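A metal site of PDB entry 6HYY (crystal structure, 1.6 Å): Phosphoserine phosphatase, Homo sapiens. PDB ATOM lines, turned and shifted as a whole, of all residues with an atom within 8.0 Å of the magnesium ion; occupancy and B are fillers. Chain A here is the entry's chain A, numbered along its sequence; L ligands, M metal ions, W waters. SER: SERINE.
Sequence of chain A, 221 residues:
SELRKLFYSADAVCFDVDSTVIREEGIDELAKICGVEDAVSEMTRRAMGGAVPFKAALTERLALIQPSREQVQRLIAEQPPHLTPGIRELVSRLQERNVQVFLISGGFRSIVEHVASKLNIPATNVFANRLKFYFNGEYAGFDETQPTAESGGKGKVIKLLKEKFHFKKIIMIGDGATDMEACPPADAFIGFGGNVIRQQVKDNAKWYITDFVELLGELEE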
ATOM      1  N   PHE A  15     -18.018  -0.603  24.294  1.00  0.00           N
ATOM      2  CA  PHE A  15     -17.220  -1.802  24.451  1.00  0.00           C
ATOM      3  C   PHE A  15     -15.750  -1.426  24.572  1.00  0.00           C
ATOM      4  O   PHE A  15     -15.223  -0.683  23.746  1.00  0.00           O
ATOM      5  CB  PHE A  15     -17.354  -2.722  23.246  1.00  0.00           C
ATOM      6  CG  PHE A  15     -18.664  -3.417  23.118  1.00  0.00           C
ATOM      7  CD1 PHE A  15     -18.894  -4.647  23.724  1.00  0.00           C
ATOM      8  CD2 PHE A  15     -19.681  -2.857  22.345  1.00  0.00           C
ATOM      9  CE1 PHE A  15     -20.099  -5.297  23.595  1.00  0.00           C
ATOM     10  CE2 PHE A  15     -20.893  -3.522  22.183  1.00  0.00           C
ATOM     11  CZ  PHE A  15     -21.122  -4.743  22.829  1.00  0.00           C
ATOM     12  N   ASP A  16     -15.087  -1.993  25.584  1.00  0.00           N
ATOM     13  CA  ASP A  16     -13.644  -2.134  25.578  1.00  0.00           C
ATOM     14  C   ASP A  16     -13.215  -2.969  24.382  1.00  0.00           C
ATOM     15  O   ASP A  16     -13.915  -3.909  24.000  1.00  0.00           O
ATOM     16  CB  ASP A  16     -13.244  -2.797  26.909  1.00  0.00           C
ATOM     17  CG  ASP A  16     -11.791  -3.217  26.957  1.00  0.00           C
ATOM     18  OD1 ASP A  16     -10.914  -2.380  26.725  1.00  0.00           O
ATOM     19  OD2 ASP A  16     -11.553  -4.395  27.270  1.00  0.00           O
ATOM     20  N   VAL A  17     -12.062  -2.651  23.796  1.00  0.00           N
ATOM     21  CA  VAL A  17     -11.584  -3.432  22.655  1.00  0.00           C
ATOM     22  C   VAL A  17     -10.698  -4.615  23.082  1.00  0.00           C
ATOM     23  O   VAL A  17     -11.076  -5.781  22.870  1.00  0.00           O
ATOM     24  CB  VAL A  17     -10.872  -2.528  21.637  1.00  0.00           C
ATOM     25  CG1 VAL A  17     -10.307  -3.367  20.489  1.00  0.00           C
ATOM     26  CG2 VAL A  17     -11.831  -1.458  21.119  1.00  0.00           C
ATOM     27  N   ASP A  18      -9.525  -4.338  23.673  1.00  0.00           N
ATOM     28  CA  ASP A  18      -8.559  -5.423  23.925  1.00  0.00           C
ATOM     29  C   ASP A  18      -9.111  -6.446  24.915  1.00  0.00           C
ATOM     30  O   ASP A  18      -9.495  -6.098  26.036  1.00  0.00           O
ATOM     31  CB  ASP A  18      -7.211  -4.914  24.469  1.00  0.00           C
ATOM     32  CG  ASP A  18      -6.425  -4.033  23.493  1.00  0.00           C
ATOM     33  OD1 ASP A  18      -6.638  -4.091  22.273  1.00  0.00           O
ATOM     34  OD2 ASP A  18      -5.555  -3.269  23.978  1.00  0.00           O
ATOM     35  N   SER A  19      -9.101  -7.712  24.508  1.00  0.00           N
ATOM     36  CA  SER A  19      -9.584  -8.866  25.246  1.00  0.00           C
ATOM     37  C   SER A  19     -11.090  -8.860  25.458  1.00  0.00           C
ATOM     38  O   SER A  19     -11.613  -9.754  26.118  1.00  0.00           O
ATOM     39  CB  SER A  19      -8.876  -9.023  26.602  1.00  0.00           C
ATOM     40  OG  SER A  19      -7.478  -9.142  26.378  1.00  0.00           O
ATOM     41  N   THR A  20     -11.815  -7.911  24.863  1.00  0.00           N
ATOM     42  CA  THR A  20     -13.279  -7.913  24.902  1.00  0.00           C
ATOM     43  C   THR A  20     -13.827  -8.055  23.492  1.00  0.00           C
ATOM     44  O   THR A  20     -14.286  -9.150  23.134  1.00  0.00           O
ATOM     45  CB  THR A  20     -13.802  -6.662  25.597  1.00  0.00           C
ATOM     46  OG1 THR A  20     -13.357  -6.700  26.958  1.00  0.00           O
ATOM     47  CG2 THR A  20     -15.301  -6.657  25.598  1.00  0.00           C
ATOM     48  N   VAL A  21     -13.761  -7.031  22.658  1.00  0.00           N
ATOM     49  CA  VAL A  21     -14.225  -7.136  21.270  1.00  0.00           C
ATOM     50  C   VAL A  21     -13.272  -7.986  20.447  1.00  0.00           C
ATOM     51  O   VAL A  21     -13.691  -8.715  19.532  1.00  0.00           O
ATOM     52  CB  VAL A  21     -14.382  -5.734  20.672  1.00  0.00           C
ATOM     53  CG1 VAL A  21     -14.628  -5.804  19.154  1.00  0.00           C
ATOM     54  CG2 VAL A  21     -15.527  -5.013  21.339  1.00  0.00           C
ATOM     55  N   ILE A  22     -11.975  -7.895  20.726  1.00  0.00           N
ATOM     56  CA  ILE A  22     -10.981  -8.755  20.081  1.00  0.00           C
ATOM     57  C   ILE A  22     -10.343  -9.670  21.123  1.00  0.00           C
ATOM     58  O   ILE A  22     -10.377  -9.400  22.316  1.00  0.00           O
ATOM     59  CB  ILE A  22      -9.909  -7.957  19.318  1.00  0.00           C
ATOM     60  CG1 ILE A  22      -9.106  -7.077  20.288  1.00  0.00           C
ATOM     61  CG2 ILE A  22     -10.542  -7.150  18.160  1.00  0.00           C
ATOM     62  CD1 ILE A  22      -7.980  -6.265  19.626  1.00  0.00           C
ATOM     63  N   GLU A  24      -7.131 -10.467  21.476  1.00  0.00           N
ATOM     64  CA  GLU A  24      -5.757 -10.087  21.797  1.00  0.00           C
ATOM     65  C   GLU A  24      -5.709  -8.683  22.395  1.00  0.00           C
ATOM     66  O   GLU A  24      -6.722  -7.984  22.493  1.00  0.00           O
ATOM     67  CB  GLU A  24      -4.892 -10.170  20.536  1.00  0.00           C
ATOM     68  CG  GLU A  24      -5.056 -11.464  19.704  1.00  0.00           C
ATOM     69  CD  GLU A  24      -6.002 -11.304  18.508  1.00  0.00           C
ATOM     70  OE1 GLU A  24      -5.897 -12.132  17.559  1.00  0.00           O
ATOM     71  OE2 GLU A  24      -6.831 -10.371  18.504  1.00  0.00           O
ATOM     72  N   GLU A  25      -4.512  -8.277  22.807  1.00  0.00           N
ATOM     73  CA  GLU A  25      -4.251  -6.884  23.172  1.00  0.00           C
ATOM     74  C   GLU A  25      -3.496  -6.251  22.013  1.00  0.00           C
ATOM     75  O   GLU A  25      -2.431  -6.743  21.606  1.00  0.00           O
ATOM     76  CB  GLU A  25      -3.438  -6.799  24.477  1.00  0.00           C
ATOM     77  CG  GLU A  25      -4.077  -7.544  25.654  1.00  0.00           C
ATOM     78  CD  GLU A  25      -4.899  -6.631  26.560  1.00  0.00           C
ATOM     79  OE1 GLU A  25      -4.317  -5.674  27.106  1.00  0.00           O
ATOM     80  OE2 GLU A  25      -6.118  -6.878  26.737  1.00  0.00           O
ATOM     81  N   ILE A 104     -14.051   1.826  22.818  1.00  0.00           N
ATOM     82  CA  ILE A 104     -13.120   2.640  23.608  1.00  0.00           C
ATOM     83  C   ILE A 104     -11.878   1.805  23.878  1.00  0.00           C
ATOM     84  O   ILE A 104     -11.977   0.654  24.304  1.00  0.00           O
ATOM     85  CB  ILE A 104     -13.745   3.112  24.942  1.00  0.00           C
ATOM     86  CG1 ILE A 104     -15.087   3.803  24.686  1.00  0.00           C
ATOM     87  CG2 ILE A 104     -12.778   4.076  25.639  1.00  0.00           C
ATOM     88  CD1 ILE A 104     -15.812   4.196  25.964  1.00  0.00           C
ATOM     89  N   SER A 105     -10.708   2.392  23.618  1.00  0.00           N
ATOM     90  CA  SER A 105      -9.501   1.601  23.757  1.00  0.00           C
ATOM     91  C   SER A 105      -8.313   2.481  24.137  1.00  0.00           C
ATOM     92  O   SER A 105      -8.192   3.608  23.678  1.00  0.00           O
ATOM     93  CB  SER A 105      -9.198   0.857  22.457  1.00  0.00           C
ATOM     94  OG  SER A 105      -8.100  -0.020  22.666  1.00  0.00           O
ATOM     95  N   GLY A 106      -7.433   1.921  24.966  1.00  0.00           N
ATOM     96  CA  GLY A 106      -6.086   2.450  25.142  1.00  0.00           C
ATOM     97  C   GLY A 106      -5.125   2.071  24.038  1.00  0.00           C
ATOM     98  O   GLY A 106      -3.983   2.560  24.028  1.00  0.00           O
ATOM     99  N   LYS A 154     -11.343   5.993  30.037  1.00  0.00           N
ATOM    100  CA  LYS A 154     -12.622   5.455  29.572  1.00  0.00           C
ATOM    101  C   LYS A 154     -13.783   6.210  30.192  1.00  0.00           C
ATOM    102  O   LYS A 154     -14.790   6.486  29.518  1.00  0.00           O
ATOM    103  CB  LYS A 154     -12.713   3.960  29.907  1.00  0.00           C
ATOM    104  CG  LYS A 154     -11.822   3.131  28.972  1.00  0.00           C
ATOM    105  CD  LYS A 154     -11.796   1.683  29.380  1.00  0.00           C
ATOM    106  CE  LYS A 154     -10.925   0.891  28.414  1.00  0.00           C
ATOM    107  NZ  LYS A 154     -10.462  -0.397  29.021  1.00  0.00           N
ATOM    108  N   MET A 172     -21.274   0.186  30.003  1.00  0.00           N
ATOM    109  CA  MET A 172     -19.887  -0.149  29.669  1.00  0.00           C
ATOM    110  C   MET A 172     -19.697  -1.662  29.759  1.00  0.00           C
ATOM    111  O   MET A 172     -20.160  -2.276  30.713  1.00  0.00           O
ATOM    112  CB  MET A 172     -18.922   0.531  30.637  1.00  0.00           C
ATOM    113  CG  MET A 172     -17.467   0.168  30.412  1.00  0.00           C
ATOM    114  SD  MET A 172     -16.760   1.114  29.057  1.00  0.00           S
ATOM    115  CE  MET A 172     -15.460   0.038  28.439  1.00  0.00           C
ATOM    116  N   ILE A 173     -19.049  -2.256  28.742  1.00  0.00           N
ATOM    117  CA  ILE A 173     -18.780  -3.699  28.694  1.00  0.00           C
ATOM    118  C   ILE A 173     -17.297  -3.907  28.513  1.00  0.00           C
ATOM    119  O   ILE A 173     -16.725  -3.406  27.538  1.00  0.00           O
ATOM    120  CB  ILE A 173     -19.576  -4.388  27.581  1.00  0.00           C
ATOM    121  CG1 ILE A 173     -21.072  -4.172  27.789  1.00  0.00           C
ATOM    122  CG2 ILE A 173     -19.192  -5.897  27.526  1.00  0.00           C
ATOM    123  CD1 ILE A 173     -21.990  -4.926  26.829  1.00  0.00           C
ATOM    124  N   GLY A 174     -16.677  -4.659  29.414  1.00  0.00           N
ATOM    125  CA  GLY A 174     -15.245  -4.893  29.291  1.00  0.00           C
ATOM    126  C   GLY A 174     -14.762  -5.921  30.282  1.00  0.00           C
ATOM    127  O   GLY A 174     -15.496  -6.367  31.168  1.00  0.00           O
ATOM    128  N   ASP A 175     -13.497  -6.320  30.101  1.00  0.00           N
ATOM    129  CA  ASP A 175     -12.933  -7.413  30.874  1.00  0.00           C
ATOM    130  C   ASP A 175     -12.162  -6.972  32.100  1.00  0.00           C
ATOM    131  O   ASP A 175     -11.935  -7.811  32.990  1.00  0.00           O
ATOM    132  CB  ASP A 175     -11.989  -8.241  29.984  1.00  0.00           C
ATOM    133  CG  ASP A 175     -10.754  -7.468  29.580  1.00  0.00           C
ATOM    134  OD1 ASP A 175     -10.906  -6.419  28.939  1.00  0.00           O
ATOM    135  OD2 ASP A 175      -9.608  -7.910  29.879  1.00  0.00           O
ATOM    136  N   GLY A 176     -11.764  -5.703  32.199  1.00  0.00           N
ATOM    137  CA  GLY A 176     -10.752  -5.293  33.153  1.00  0.00           C
ATOM    138  C   GLY A 176     -11.256  -4.308  34.196  1.00  0.00           C
ATOM    139  O   GLY A 176     -12.361  -3.771  34.114  1.00  0.00           O
ATOM    140  N   ALA A 177     -10.402  -4.086  35.202  1.00  0.00           N
ATOM    141  CA  ALA A 177     -10.791  -3.168  36.268  1.00  0.00           C
ATOM    142  C   ALA A 177     -10.994  -1.741  35.758  1.00  0.00           C
ATOM    143  O   ALA A 177     -11.875  -1.027  36.254  1.00  0.00           O
ATOM    144  CB  ALA A 177      -9.733  -3.201  37.384  1.00  0.00           C
ATOM    145  N   THR A 178     -10.219  -1.321  34.747  1.00  0.00           N
ATOM    146  CA  THR A 178     -10.419   0.025  34.204  1.00  0.00           C
ATOM    147  C   THR A 178     -11.792   0.159  33.542  1.00  0.00           C
ATOM    148  O   THR A 178     -12.349   1.259  33.516  1.00  0.00           O
ATOM    149  CB  THR A 178      -9.316   0.400  33.210  1.00  0.00           C
ATOM    150  OG1 THR A 178      -9.390  -0.441  32.042  1.00  0.00           O
ATOM    151  CG2 THR A 178      -7.956   0.273  33.868  1.00  0.00           C
ATOM    152  N   ASP A 179     -12.352  -0.930  33.027  1.00  0.00           N
ATOM    153  CA  ASP A 179     -13.710  -0.892  32.513  1.00  0.00           C
ATOM    154  C   ASP A 179     -14.731  -0.795  33.642  1.00  0.00           C
ATOM    155  O   ASP A 179     -15.670   0.001  33.588  1.00  0.00           O
ATOM    156  CB  ASP A 179     -13.956  -2.150  31.658  1.00  0.00           C
ATOM    157  CG  ASP A 179     -12.912  -2.311  30.603  1.00  0.00           C
ATOM    158  OD1 ASP A 179     -12.792  -1.404  29.777  1.00  0.00           O
ATOM    159  OD2 ASP A 179     -12.180  -3.332  30.607  1.00  0.00           O
ATOM    160  N   PHE A 192     -16.784  -8.956  31.228  1.00  0.00           N
ATOM    161  CA  PHE A 192     -16.698  -9.970  30.173  1.00  0.00           C
ATOM    162  C   PHE A 192     -15.480 -10.859  30.362  1.00  0.00           C
ATOM    163  O   PHE A 192     -14.347 -10.367  30.331  1.00  0.00           O
ATOM    164  CB  PHE A 192     -16.641  -9.304  28.789  1.00  0.00           C
ATOM    165  CG  PHE A 192     -16.591 -10.306  27.682  1.00  0.00           C
ATOM    166  CD1 PHE A 192     -17.717 -11.049  27.343  1.00  0.00           C
ATOM    167  CD2 PHE A 192     -15.416 -10.524  26.995  1.00  0.00           C
ATOM    168  CE1 PHE A 192     -17.676 -11.979  26.349  1.00  0.00           C
ATOM    169  CE2 PHE A 192     -15.364 -11.488  25.981  1.00  0.00           C
ATOM    170  CZ  PHE A 192     -16.496 -12.205  25.659  1.00  0.00           C
ATOM    171  N   ARG A 198     -10.713 -11.986  34.447  1.00  0.00           N
ATOM    172  CA  ARG A 198      -9.996 -11.252  35.488  1.00  0.00           C
ATOM    173  C   ARG A 198     -10.819 -11.415  36.764  1.00  0.00           C
ATOM    174  O   ARG A 198     -11.882 -10.820  36.904  1.00  0.00           O
ATOM    175  CB  ARG A 198      -9.788  -9.806  35.070  1.00  0.00           C
ATOM    176  CG  ARG A 198      -8.633  -9.667  34.078  1.00  0.00           C
ATOM    177  CD  ARG A 198      -8.787  -8.534  33.090  1.00  0.00           C
ATOM    178  NE  ARG A 198      -8.298  -8.916  31.765  1.00  0.00           N
ATOM    179  CZ  ARG A 198      -7.033  -8.836  31.366  1.00  0.00           C
ATOM    180  NH1 ARG A 198      -6.094  -8.402  32.188  1.00  0.00           N
ATOM    181  NH2 ARG A 198      -6.697  -9.207  30.140  1.00  0.00           N
HETATM  182  N   SER L   1      -5.787  -1.427  25.704  1.00  0.00           N
HETATM  183  CA  SER L   1      -7.157  -0.928  25.758  1.00  0.00           C
HETATM  184  C   SER L   1      -7.439  -0.303  27.115  1.00  0.00           C
HETATM  185  O   SER L   1      -8.437  -0.659  27.736  1.00  0.00           O
HETATM  186  CB  SER L   1      -8.146  -2.056  25.521  1.00  0.00           C
HETATM  187  OG  SER L   1      -9.333  -1.636  24.877  1.00  0.00           O
HETATM  188  OXT SER L   1      -6.697   0.535  27.633  1.00  0.00           O
HETATM  189 MG    MG M   1      -9.532  -4.879  27.976  1.00  0.00          MG
HETATM  190  O   HOH W   1      -9.623  -3.597  29.801  1.00  0.00           O
HETATM  191  O   HOH W   2      -7.925  -3.643  27.829  1.00  0.00           O
HETATM  192  O   HOH W   3      -7.869  -6.216  28.684  1.00  0.00           O
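An oxygen (OG) of the ligand lies within hydrogen-bond range of the side-chain carboxylate (OD1) of Asp 16 (2.5 Å). The backbone NH of Asp 18 lies within hydrogen-bond range of an oxygen (OG) of the ligand, 3.0 Å away. A nitrogen (N) of the ligand lies within salt-bridge range of the side-chain carboxylate of Asp 18 (2.5 Å). The side-chain amino group (NZ) of Lys 154 is in salt-bridge range of an oxygen (O) of the ligand. An oxygen (OG) of the ligand is in hydrogen-bond range of the backbone NH of Val 17 (3.1 Å). The side-chain hydroxyl (OG) of Ser 105 is in hydrogen-bond range of an oxygen (OG) of the ligand (3.0 Å). The backbone NH (N) of Gly 106 lies close to an oxygen (OXT) of the ligand (3.1 Å).
OD2 of Asp 16 lies close to OG1 of Thr 20 (2.9 Å). The side-chain carboxylate (OD1) of Asp 16 is in salt-bridge range of the side-chain amino group (NZ) of Lys 154 (3.1 Å). The backbone carbonyl oxygen (O) of Asp 16 lies close to the backbone NH (N) of Val 21, 3.4 Å away. O of Ile 173 sits at hydrogen-bond distance from N of Asp 16 (2.9 Å). The backbone NH of Asp 175 sits at hydrogen-bond distance from the side-chain carboxylate of Asp 179, at 3.3 Å. The backbone NH (N) of Asp 175 lies within hydrogen-bond range of the side-chain hydroxyl (OG1) of Thr 20 (3.2 Å). OD2 of Asp 175 lies within salt-bridge range of NE of Arg 198 (2.5 Å).
Within 4 Å of the magnesium ion: Asp 16, Asp 18 and Asp 175.
The magnesium ion is bound by water W2 (2.0 Å), OD2 of Asp 16 (2.2 Å), water W1 (2.2 Å), water W3 (2.2 Å), OD1 of Asp 175 (2.3 Å) and O of Asp 18 (2.3 Å).
Water W2 bridges an oxygen (O) of the ligand (3.0 Å) and the side-chain carboxylate (OD1) of Asp 16 (3.4 Å). Water W1 lies within hydrogen-bond range of the side-chain carboxylate (OD2) of Asp 179 and the side-chain amino group (NZ) of Lys 154. Water W3 lies within hydrogen-bond range of the side-chain carboxylate (OE2) of Glu 25 (2.7 Å) and the side-chain carboxylate (OD2) of Asp 175 (2.7 Å).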
